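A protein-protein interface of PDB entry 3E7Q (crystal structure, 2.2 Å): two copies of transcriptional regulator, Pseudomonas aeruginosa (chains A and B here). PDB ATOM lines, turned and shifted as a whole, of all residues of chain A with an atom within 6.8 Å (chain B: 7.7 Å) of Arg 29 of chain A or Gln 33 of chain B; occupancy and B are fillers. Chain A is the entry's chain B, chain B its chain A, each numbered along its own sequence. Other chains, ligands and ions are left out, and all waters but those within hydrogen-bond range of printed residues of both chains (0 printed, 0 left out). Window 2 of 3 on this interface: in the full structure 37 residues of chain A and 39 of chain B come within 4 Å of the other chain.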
ATOM      1  N   LEU A  24      -7.024 -29.690  -2.454  1.00  0.00           N
ATOM      2  CA  LEU A  24      -6.973 -29.382  -1.021  1.00  0.00           C
ATOM      3  C   LEU A  24      -6.196 -28.081  -0.689  1.00  0.00           C
ATOM      4  O   LEU A  24      -6.559 -27.366   0.257  1.00  0.00           O
ATOM      5  CB  LEU A  24      -6.420 -30.555  -0.217  1.00  0.00           C
ATOM      6  CG  LEU A  24      -7.233 -31.866  -0.275  1.00  0.00           C
ATOM      7  CD1 LEU A  24      -6.329 -32.988   0.189  1.00  0.00           C
ATOM      8  CD2 LEU A  24      -8.557 -31.731   0.522  1.00  0.00           C
ATOM      9  N   ALA A  25      -5.156 -27.792  -1.465  1.00  0.00           N
ATOM     10  CA  ALA A  25      -4.274 -26.620  -1.276  1.00  0.00           C
ATOM     11  C   ALA A  25      -4.972 -25.392  -1.726  1.00  0.00           C
ATOM     12  O   ALA A  25      -4.929 -24.359  -1.063  1.00  0.00           O
ATOM     13  CB  ALA A  25      -2.883 -26.775  -2.062  1.00  0.00           C
ATOM     14  N   CYS A  26      -5.636 -25.502  -2.864  1.00  0.00           N
ATOM     15  CA  CYS A  26      -6.511 -24.428  -3.303  1.00  0.00           C
ATOM     16  C   CYS A  26      -7.661 -24.088  -2.339  1.00  0.00           C
ATOM     17  O   CYS A  26      -7.971 -22.891  -2.159  1.00  0.00           O
ATOM     18  CB  CYS A  26      -7.061 -24.742  -4.670  1.00  0.00           C
ATOM     19  SG  CYS A  26      -8.162 -23.489  -5.221  1.00  0.00           S
ATOM     20  N   LEU A  27      -8.297 -25.110  -1.741  1.00  0.00           N
ATOM     21  CA  LEU A  27      -9.351 -24.882  -0.781  1.00  0.00           C
ATOM     22  C   LEU A  27      -8.848 -24.169   0.479  1.00  0.00           C
ATOM     23  O   LEU A  27      -9.543 -23.302   1.034  1.00  0.00           O
ATOM     24  CB  LEU A  27     -10.000 -26.202  -0.359  1.00  0.00           C
ATOM     25  CG  LEU A  27     -10.853 -26.963  -1.365  1.00  0.00           C
ATOM     26  CD1 LEU A  27     -11.141 -28.324  -0.788  1.00  0.00           C
ATOM     27  CD2 LEU A  27     -12.148 -26.218  -1.788  1.00  0.00           C
ATOM     28  N   LYS A  28      -7.657 -24.569   0.934  1.00  0.00           N
ATOM     29  CA  LYS A  28      -6.999 -23.984   2.096  1.00  0.00           C
ATOM     30  C   LYS A  28      -6.611 -22.549   1.851  1.00  0.00           C
ATOM     31  O   LYS A  28      -6.600 -21.791   2.805  1.00  0.00           O
ATOM     32  CB  LYS A  28      -5.774 -24.819   2.543  1.00  0.00           C
ATOM     33  CG  LYS A  28      -4.805 -24.117   3.557  1.00  0.00           C
ATOM     34  CD  LYS A  28      -4.064 -25.104   4.479  1.00  0.00           C
ATOM     35  CE  LYS A  28      -2.930 -24.375   5.276  1.00  0.00           C
ATOM     36  NZ  LYS A  28      -2.364 -25.182   6.438  1.00  0.00           N
ATOM     37  N   ARG A  29      -6.373 -22.160   0.593  1.00  0.00           N
ATOM     38  CA  ARG A  29      -5.958 -20.787   0.251  1.00  0.00           C
ATOM     39  C   ARG A  29      -7.082 -19.848  -0.227  1.00  0.00           C
ATOM     40  O   ARG A  29      -7.016 -18.634  -0.007  1.00  0.00           O
ATOM     41  CB  ARG A  29      -4.869 -20.843  -0.837  1.00  0.00           C
ATOM     42  CG  ARG A  29      -4.588 -19.545  -1.584  1.00  0.00           C
ATOM     43  CD  ARG A  29      -3.691 -19.814  -2.717  1.00  0.00           C
ATOM     44  NE  ARG A  29      -2.394 -20.308  -2.251  1.00  0.00           N
ATOM     45  CZ  ARG A  29      -1.258 -19.598  -2.224  1.00  0.00           C
ATOM     46  NH1 ARG A  29      -1.223 -18.330  -2.641  1.00  0.00           N
ATOM     47  NH2 ARG A  29      -0.139 -20.170  -1.770  1.00  0.00           N
ATOM     48  N   HIS A  30      -8.105 -20.378  -0.889  1.00  0.00           N
ATOM     49  CA  HIS A  30      -9.112 -19.523  -1.468  1.00  0.00           C
ATOM     50  C   HIS A  30     -10.471 -19.735  -0.885  1.00  0.00           C
ATOM     51  O   HIS A  30     -11.395 -19.011  -1.231  1.00  0.00           O
ATOM     52  CB  HIS A  30      -9.182 -19.733  -2.977  1.00  0.00           C
ATOM     53  CG  HIS A  30      -7.905 -19.419  -3.677  1.00  0.00           C
ATOM     54  ND1 HIS A  30      -7.382 -18.141  -3.728  1.00  0.00           N
ATOM     55  CD2 HIS A  30      -7.033 -20.215  -4.342  1.00  0.00           C
ATOM     56  CE1 HIS A  30      -6.249 -18.164  -4.407  1.00  0.00           C
ATOM     57  NE2 HIS A  30      -6.016 -19.407  -4.797  1.00  0.00           N
ATOM     58  N   GLY A  31     -10.624 -20.733  -0.028  1.00  0.00           N
ATOM     59  CA  GLY A  31     -11.964 -21.250   0.292  1.00  0.00           C
ATOM     60  C   GLY A  31     -12.654 -21.969  -0.875  1.00  0.00           C
ATOM     61  O   GLY A  31     -12.212 -21.944  -2.018  1.00  0.00           O
ATOM     62  N   PHE A  32     -13.770 -22.619  -0.575  1.00  0.00           N
ATOM     63  CA  PHE A  32     -14.550 -23.256  -1.635  1.00  0.00           C
ATOM     64  C   PHE A  32     -15.101 -22.258  -2.595  1.00  0.00           C
ATOM     65  O   PHE A  32     -15.027 -22.471  -3.800  1.00  0.00           O
ATOM     66  CB  PHE A  32     -15.704 -24.083  -1.103  1.00  0.00           C
ATOM     67  CG  PHE A  32     -16.618 -24.614  -2.196  1.00  0.00           C
ATOM     68  CD1 PHE A  32     -16.266 -25.717  -2.935  1.00  0.00           C
ATOM     69  CD2 PHE A  32     -17.834 -23.976  -2.491  1.00  0.00           C
ATOM     70  CE1 PHE A  32     -17.109 -26.206  -3.940  1.00  0.00           C
ATOM     71  CE2 PHE A  32     -18.659 -24.444  -3.520  1.00  0.00           C
ATOM     72  CZ  PHE A  32     -18.311 -25.574  -4.219  1.00  0.00           C
ATOM     73  N   GLN A  33     -15.675 -21.179  -2.068  1.00  0.00           N
ATOM     74  CA  GLN A  33     -16.293 -20.165  -2.951  1.00  0.00           C
ATOM     75  C   GLN A  33     -15.237 -19.558  -3.891  1.00  0.00           C
ATOM     76  O   GLN A  33     -15.515 -19.268  -5.065  1.00  0.00           O
ATOM     77  CB  GLN A  33     -16.993 -19.042  -2.150  1.00  0.00           C
ATOM     78  CG  GLN A  33     -18.040 -19.493  -1.151  1.00  0.00           C
ATOM     79  CD  GLN A  33     -17.450 -19.688   0.269  1.00  0.00           C
ATOM     80  OE1 GLN A  33     -16.292 -20.134   0.412  1.00  0.00           O
ATOM     81  NE2 GLN A  33     -18.247 -19.372   1.311  1.00  0.00           N
ATOM     82  N   GLY A  34     -14.027 -19.350  -3.376  1.00  0.00           N
ATOM     83  CA  GLY A  34     -12.982 -18.748  -4.198  1.00  0.00           C
ATOM     84  C   GLY A  34     -12.178 -19.684  -5.096  1.00  0.00           C
ATOM     85  O   GLY A  34     -11.487 -19.212  -5.989  1.00  0.00           O
ATOM     86  N   LYS A  39      -7.456 -22.010 -10.466  1.00  0.00           N
ATOM     87  CA  LYS A  39      -6.713 -21.934  -9.215  1.00  0.00           C
ATOM     88  C   LYS A  39      -6.241 -23.299  -8.645  1.00  0.00           C
ATOM     89  O   LYS A  39      -5.259 -23.346  -7.864  1.00  0.00           O
ATOM     90  CB  LYS A  39      -7.500 -21.155  -8.168  1.00  0.00           C
ATOM     91  CG  LYS A  39      -7.651 -19.673  -8.481  1.00  0.00           C
ATOM     92  CD  LYS A  39      -8.627 -19.038  -7.479  1.00  0.00           C
ATOM     93  CE  LYS A  39      -8.548 -17.499  -7.459  1.00  0.00           C
ATOM     94  NZ  LYS A  39      -9.589 -16.870  -6.539  1.00  0.00           N
ATOM     95  N   GLU A  43      -2.108 -24.682  -8.150  1.00  0.00           N
ATOM     96  CA  GLU A  43      -1.488 -25.472  -7.088  1.00  0.00           C
ATOM     97  C   GLU A  43      -0.773 -26.671  -7.683  1.00  0.00           C
ATOM     98  O   GLU A  43       0.361 -26.906  -7.326  1.00  0.00           O
ATOM     99  CB  GLU A  43      -2.504 -25.886  -6.035  1.00  0.00           C
ATOM    100  CG  GLU A  43      -3.235 -24.683  -5.352  1.00  0.00           C
ATOM    101  CD  GLU A  43      -2.300 -23.712  -4.574  1.00  0.00           C
ATOM    102  OE1 GLU A  43      -1.238 -24.165  -4.060  1.00  0.00           O
ATOM    103  OE2 GLU A  43      -2.643 -22.505  -4.462  1.00  0.00           O
ATOM    104  N   ASP A 111      -8.815 -26.676   7.660  1.00  0.00           N
ATOM    105  CA  ASP A 111      -9.248 -25.764   6.619  1.00  0.00           C
ATOM    106  C   ASP A 111     -10.000 -26.469   5.487  1.00  0.00           C
ATOM    107  O   ASP A 111     -10.944 -25.898   4.907  1.00  0.00           O
ATOM    108  CB  ASP A 111      -8.041 -25.007   6.008  1.00  0.00           C
ATOM    109  CG  ASP A 111      -6.887 -24.740   7.025  1.00  0.00           C
ATOM    110  OD1 ASP A 111      -6.527 -23.522   7.160  1.00  0.00           O
ATOM    111  OD2 ASP A 111      -6.344 -25.727   7.634  1.00  0.00           O
ATOM    112  N   CYS B  26     -21.494 -11.348   2.442  1.00  0.00           N
ATOM    113  CA  CYS B  26     -20.244 -11.514   1.690  1.00  0.00           C
ATOM    114  C   CYS B  26     -19.355 -12.720   2.135  1.00  0.00           C
ATOM    115  O   CYS B  26     -18.734 -13.395   1.294  1.00  0.00           O
ATOM    116  CB  CYS B  26     -19.447 -10.239   1.814  1.00  0.00           C
ATOM    117  SG  CYS B  26     -20.247  -8.893   0.928  1.00  0.00           S
ATOM    118  N   LEU B  27     -19.289 -12.959   3.445  1.00  0.00           N
ATOM    119  CA  LEU B  27     -18.632 -14.163   3.951  1.00  0.00           C
ATOM    120  C   LEU B  27     -19.361 -15.407   3.398  1.00  0.00           C
ATOM    121  O   LEU B  27     -18.730 -16.319   2.910  1.00  0.00           O
ATOM    122  CB  LEU B  27     -18.611 -14.224   5.496  1.00  0.00           C
ATOM    123  CG  LEU B  27     -17.692 -13.234   6.206  1.00  0.00           C
ATOM    124  CD1 LEU B  27     -18.033 -13.271   7.784  1.00  0.00           C
ATOM    125  CD2 LEU B  27     -16.248 -13.557   5.838  1.00  0.00           C
ATOM    126  N   HIS B  30     -18.539 -15.277  -0.589  1.00  0.00           N
ATOM    127  CA  HIS B  30     -17.181 -15.240  -1.048  1.00  0.00           C
ATOM    128  C   HIS B  30     -16.153 -15.933  -0.169  1.00  0.00           C
ATOM    129  O   HIS B  30     -14.984 -16.012  -0.570  1.00  0.00           O
ATOM    130  CB  HIS B  30     -16.757 -13.788  -1.222  1.00  0.00           C
ATOM    131  CG  HIS B  30     -17.603 -13.051  -2.194  1.00  0.00           C
ATOM    132  ND1 HIS B  30     -17.528 -13.276  -3.551  1.00  0.00           N
ATOM    133  CD2 HIS B  30     -18.566 -12.124  -2.011  1.00  0.00           C
ATOM    134  CE1 HIS B  30     -18.398 -12.489  -4.158  1.00  0.00           C
ATOM    135  NE2 HIS B  30     -19.034 -11.780  -3.248  1.00  0.00           N
ATOM    136  N   GLY B  31     -16.581 -16.410   0.998  1.00  0.00           N
ATOM    137  CA  GLY B  31     -15.674 -16.934   1.980  1.00  0.00           C
ATOM    138  C   GLY B  31     -14.907 -15.772   2.612  1.00  0.00           C
ATOM    139  O   GLY B  31     -14.940 -14.624   2.114  1.00  0.00           O
ATOM    140  N   PHE B  32     -14.213 -16.070   3.706  1.00  0.00           N
ATOM    141  CA  PHE B  32     -13.411 -15.065   4.368  1.00  0.00           C
ATOM    142  C   PHE B  32     -12.344 -14.489   3.422  1.00  0.00           C
ATOM    143  O   PHE B  32     -12.079 -13.289   3.429  1.00  0.00           O
ATOM    144  CB  PHE B  32     -12.741 -15.610   5.645  1.00  0.00           C
ATOM    145  CG  PHE B  32     -11.750 -14.625   6.254  1.00  0.00           C
ATOM    146  CD1 PHE B  32     -12.200 -13.598   7.097  1.00  0.00           C
ATOM    147  CD2 PHE B  32     -10.388 -14.677   5.922  1.00  0.00           C
ATOM    148  CE1 PHE B  32     -11.310 -12.651   7.660  1.00  0.00           C
ATOM    149  CE2 PHE B  32      -9.489 -13.751   6.464  1.00  0.00           C
ATOM    150  CZ  PHE B  32      -9.951 -12.730   7.344  1.00  0.00           C
ATOM    151  N   GLN B  33     -11.716 -15.338   2.614  1.00  0.00           N
ATOM    152  CA  GLN B  33     -10.628 -14.853   1.748  1.00  0.00           C
ATOM    153  C   GLN B  33     -11.148 -13.960   0.621  1.00  0.00           C
ATOM    154  O   GLN B  33     -10.409 -13.166   0.121  1.00  0.00           O
ATOM    155  CB  GLN B  33      -9.837 -16.006   1.128  1.00  0.00           C
ATOM    156  CG  GLN B  33      -9.214 -16.999   2.125  1.00  0.00           C
ATOM    157  CD  GLN B  33     -10.129 -18.201   2.423  1.00  0.00           C
ATOM    158  OE1 GLN B  33     -11.385 -18.107   2.408  1.00  0.00           O
ATOM    159  NE2 GLN B  33      -9.509 -19.321   2.728  1.00  0.00           N
ATOM    160  N   GLY B  34     -12.394 -14.115   0.192  1.00  0.00           N
ATOM    161  CA  GLY B  34     -12.921 -13.291  -0.883  1.00  0.00           C
ATOM    162  C   GLY B  34     -13.640 -12.046  -0.435  1.00  0.00           C
ATOM    163  O   GLY B  34     -13.835 -11.090  -1.223  1.00  0.00           O
ATOM    164  N   ALA B  35     -14.040 -12.026   0.832  1.00  0.00           N
ATOM    165  CA  ALA B  35     -14.632 -10.840   1.370  1.00  0.00           C
ATOM    166  C   ALA B  35     -13.565  -9.757   1.232  1.00  0.00           C
ATOM    167  O   ALA B  35     -12.313 -10.026   1.292  1.00  0.00           O
ATOM    168  CB  ALA B  35     -15.119 -11.069   2.824  1.00  0.00           C
ATOM    169  N   SER B  36     -14.012  -8.576   0.856  1.00  0.00           N
ATOM    170  CA  SER B  36     -13.131  -7.376   0.823  1.00  0.00           C
ATOM    171  C   SER B  36     -13.990  -6.280   1.407  1.00  0.00           C
ATOM    172  O   SER B  36     -15.207  -6.453   1.489  1.00  0.00           O
ATOM    173  CB  SER B  36     -12.687  -7.037  -0.608  1.00  0.00           C
ATOM    174  OG  SER B  36     -13.794  -6.846  -1.474  1.00  0.00           O
ATOM    175  N   LYS B  39     -16.393  -5.207  -1.422  1.00  0.00           N
ATOM    176  CA  LYS B  39     -17.614  -6.030  -1.579  1.00  0.00           C
ATOM    177  C   LYS B  39     -18.644  -5.748  -0.479  1.00  0.00           C
ATOM    178  O   LYS B  39     -19.852  -5.579  -0.753  1.00  0.00           O
ATOM    179  CB  LYS B  39     -17.284  -7.520  -1.623  1.00  0.00           C
ATOM    180  CG  LYS B  39     -16.631  -7.886  -2.920  1.00  0.00           C
ATOM    181  CD  LYS B  39     -16.262  -9.349  -3.014  1.00  0.00           C
ATOM    182  CE  LYS B  39     -15.028  -9.550  -3.875  1.00  0.00           C
ATOM    183  NZ  LYS B  39     -14.778 -10.980  -3.858  1.00  0.00           N
ATOM    184  N   LYS B  58     -11.107  -5.350   6.262  1.00  0.00           N
ATOM    185  CA  LYS B  58     -11.875  -6.580   6.246  1.00  0.00           C
ATOM    186  C   LYS B  58     -11.788  -7.297   7.593  1.00  0.00           C
ATOM    187  O   LYS B  58     -12.814  -7.677   8.124  1.00  0.00           O
ATOM    188  CB  LYS B  58     -11.418  -7.503   5.086  1.00  0.00           C
ATOM    189  CG  LYS B  58     -11.644  -9.003   5.351  1.00  0.00           C
ATOM    190  CD  LYS B  58     -11.568  -9.908   4.105  1.00  0.00           C
ATOM    191  CE  LYS B  58     -10.321 -10.751   4.029  1.00  0.00           C
ATOM    192  NZ  LYS B  58     -10.208 -11.457   2.712  1.00  0.00           N
ATOM    193  N   ALA B 115     -16.814 -19.835   7.921  1.00  0.00           N
ATOM    194  CA  ALA B 115     -15.890 -18.774   7.501  1.00  0.00           C
ATOM    195  C   ALA B 115     -15.130 -18.204   8.717  1.00  0.00           C
ATOM    196  O   ALA B 115     -13.947 -18.017   8.654  1.00  0.00           O
ATOM    197  CB  ALA B 115     -16.667 -17.623   6.711  1.00  0.00           C
ATOM    198  N   GLY B 118     -12.538 -20.859   9.908  1.00  0.00           N
ATOM    199  CA  GLY B 118     -11.402 -20.825   9.008  1.00  0.00           C
ATOM    200  C   GLY B 118     -10.400 -19.698   9.220  1.00  0.00           C
ATOM    201  O   GLY B 118      -9.191 -19.865   9.016  1.00  0.00           O
ATOM    202  N   ALA B 119     -10.893 -18.532   9.599  1.00  0.00           N
ATOM    203  CA  ALA B 119     -10.049 -17.357   9.790  1.00  0.00           C
ATOM    204  C   ALA B 119      -9.374 -17.351  11.162  1.00  0.00           C
ATOM    205  O   ALA B 119      -8.445 -16.581  11.398  1.00  0.00           O
ATOM    206  CB  ALA B 119     -10.882 -16.102   9.629  1.00  0.00           C
ATOM    207  N   SER B 122      -5.434 -17.750  11.359  1.00  0.00           N
ATOM    208  CA  SER B 122      -4.622 -16.786  10.620  1.00  0.00           C
ATOM    209  C   SER B 122      -4.713 -15.418  11.253  1.00  0.00           C
ATOM    210  O   SER B 122      -3.699 -14.802  11.466  1.00  0.00           O
ATOM    211  CB  SER B 122      -5.140 -16.703   9.181  1.00  0.00           C
ATOM    212  OG  SER B 122      -5.855 -17.895   8.853  1.00  0.00           O
ATOM    213  N   ILE B 123      -5.924 -14.950  11.550  1.00  0.00           N
ATOM    214  CA  ILE B 123      -6.165 -13.568  11.935  1.00  0.00           C
ATOM    215  C   ILE B 123      -6.366 -13.492  13.434  1.00  0.00           C
ATOM    216  O   ILE B 123      -7.301 -14.103  13.987  1.00  0.00           O
ATOM    217  CB  ILE B 123      -7.399 -12.968  11.192  1.00  0.00           C
ATOM    218  CG1 ILE B 123      -7.244 -13.149   9.696  1.00  0.00           C
ATOM    219  CG2 ILE B 123      -7.594 -11.484  11.499  1.00  0.00           C
ATOM    220  CD1 ILE B 123      -7.885 -14.399   9.204  1.00  0.00           C
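The backbone carbonyl oxygen (O) of Gln 33 of chain B lies within hydrogen-bond range of the side-chain amino group (NZ) of Lys 58 of chain B. The guanidinium group of Arg 29 of chain A lies within salt-bridge range of the side-chain carboxylate of Glu 43 of chain A (3.1 Å).
His 30 of chain A touches Gln 33 of chain B, and with the chains exchanged Gln 33 of chain A touches His 30 of chain B. Gly 31 of chain A touches Gln 33 of chain B, and with the chains exchanged Gln 33 of chain A touches Gly 31 of chain B. Gln 33 of chain A touches Leu 27 of chain B, but with the chains exchanged Leu 27 of chain A does not touch Gln 33 of chain B (4.3 Å). Of the 7 pairs that touch across the chains among the printed residues, 4 have their exchanged pair printed and touching as well.
Of the 14 printed residues of chain A, 5 touch a printed residue of chain B. Printed residues of chain A that touch a printed residue of chain B: Lys 28, Arg 29, His 30, Gly 31 and Gln 33.
O of Lys 28 of chain A touches NE2 of Gln 33 of chain B, at 3.8 Å. Arg 29 of chain A touches Gln 33 of chain B. His 30 of chain A touches Gln 33 of chain B (C to CD, 3.7 Å). His 30 of chain B touches Gln 33 of chain A.
Ala 25 of chain A touches none of the printed residues of chain B. Arg 29 of chain A touches one residue of chain B. Of the printed residues of chain B, Gln 33 of chain A touches Leu 27, His 30 and Gly 31. Glu 43 of chain A touches none of the printed residues of chain B. Printed residues of chain A within 4 Å of His 30 of chain B: Gln 33. Gln 33 of chain B touches four residues of chain A. The nearest printed residue of chain A that does not touch Leu 27 of chain B is Gly 34 of chain A (8.4 Å).
The backbone carbonyl oxygen of Leu 27 of chain B sits at hydrogen-bond distance from the side-chain amide nitrogen of Gln 33 of chain A (3.5 Å). N of Gly 31 of chain B sits close to NE2 of Gln 33 of chain A (3.4 Å). N of Gly 31 of chain A sits close to NE2 of Gln 33 of chain B (3.3 Å).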
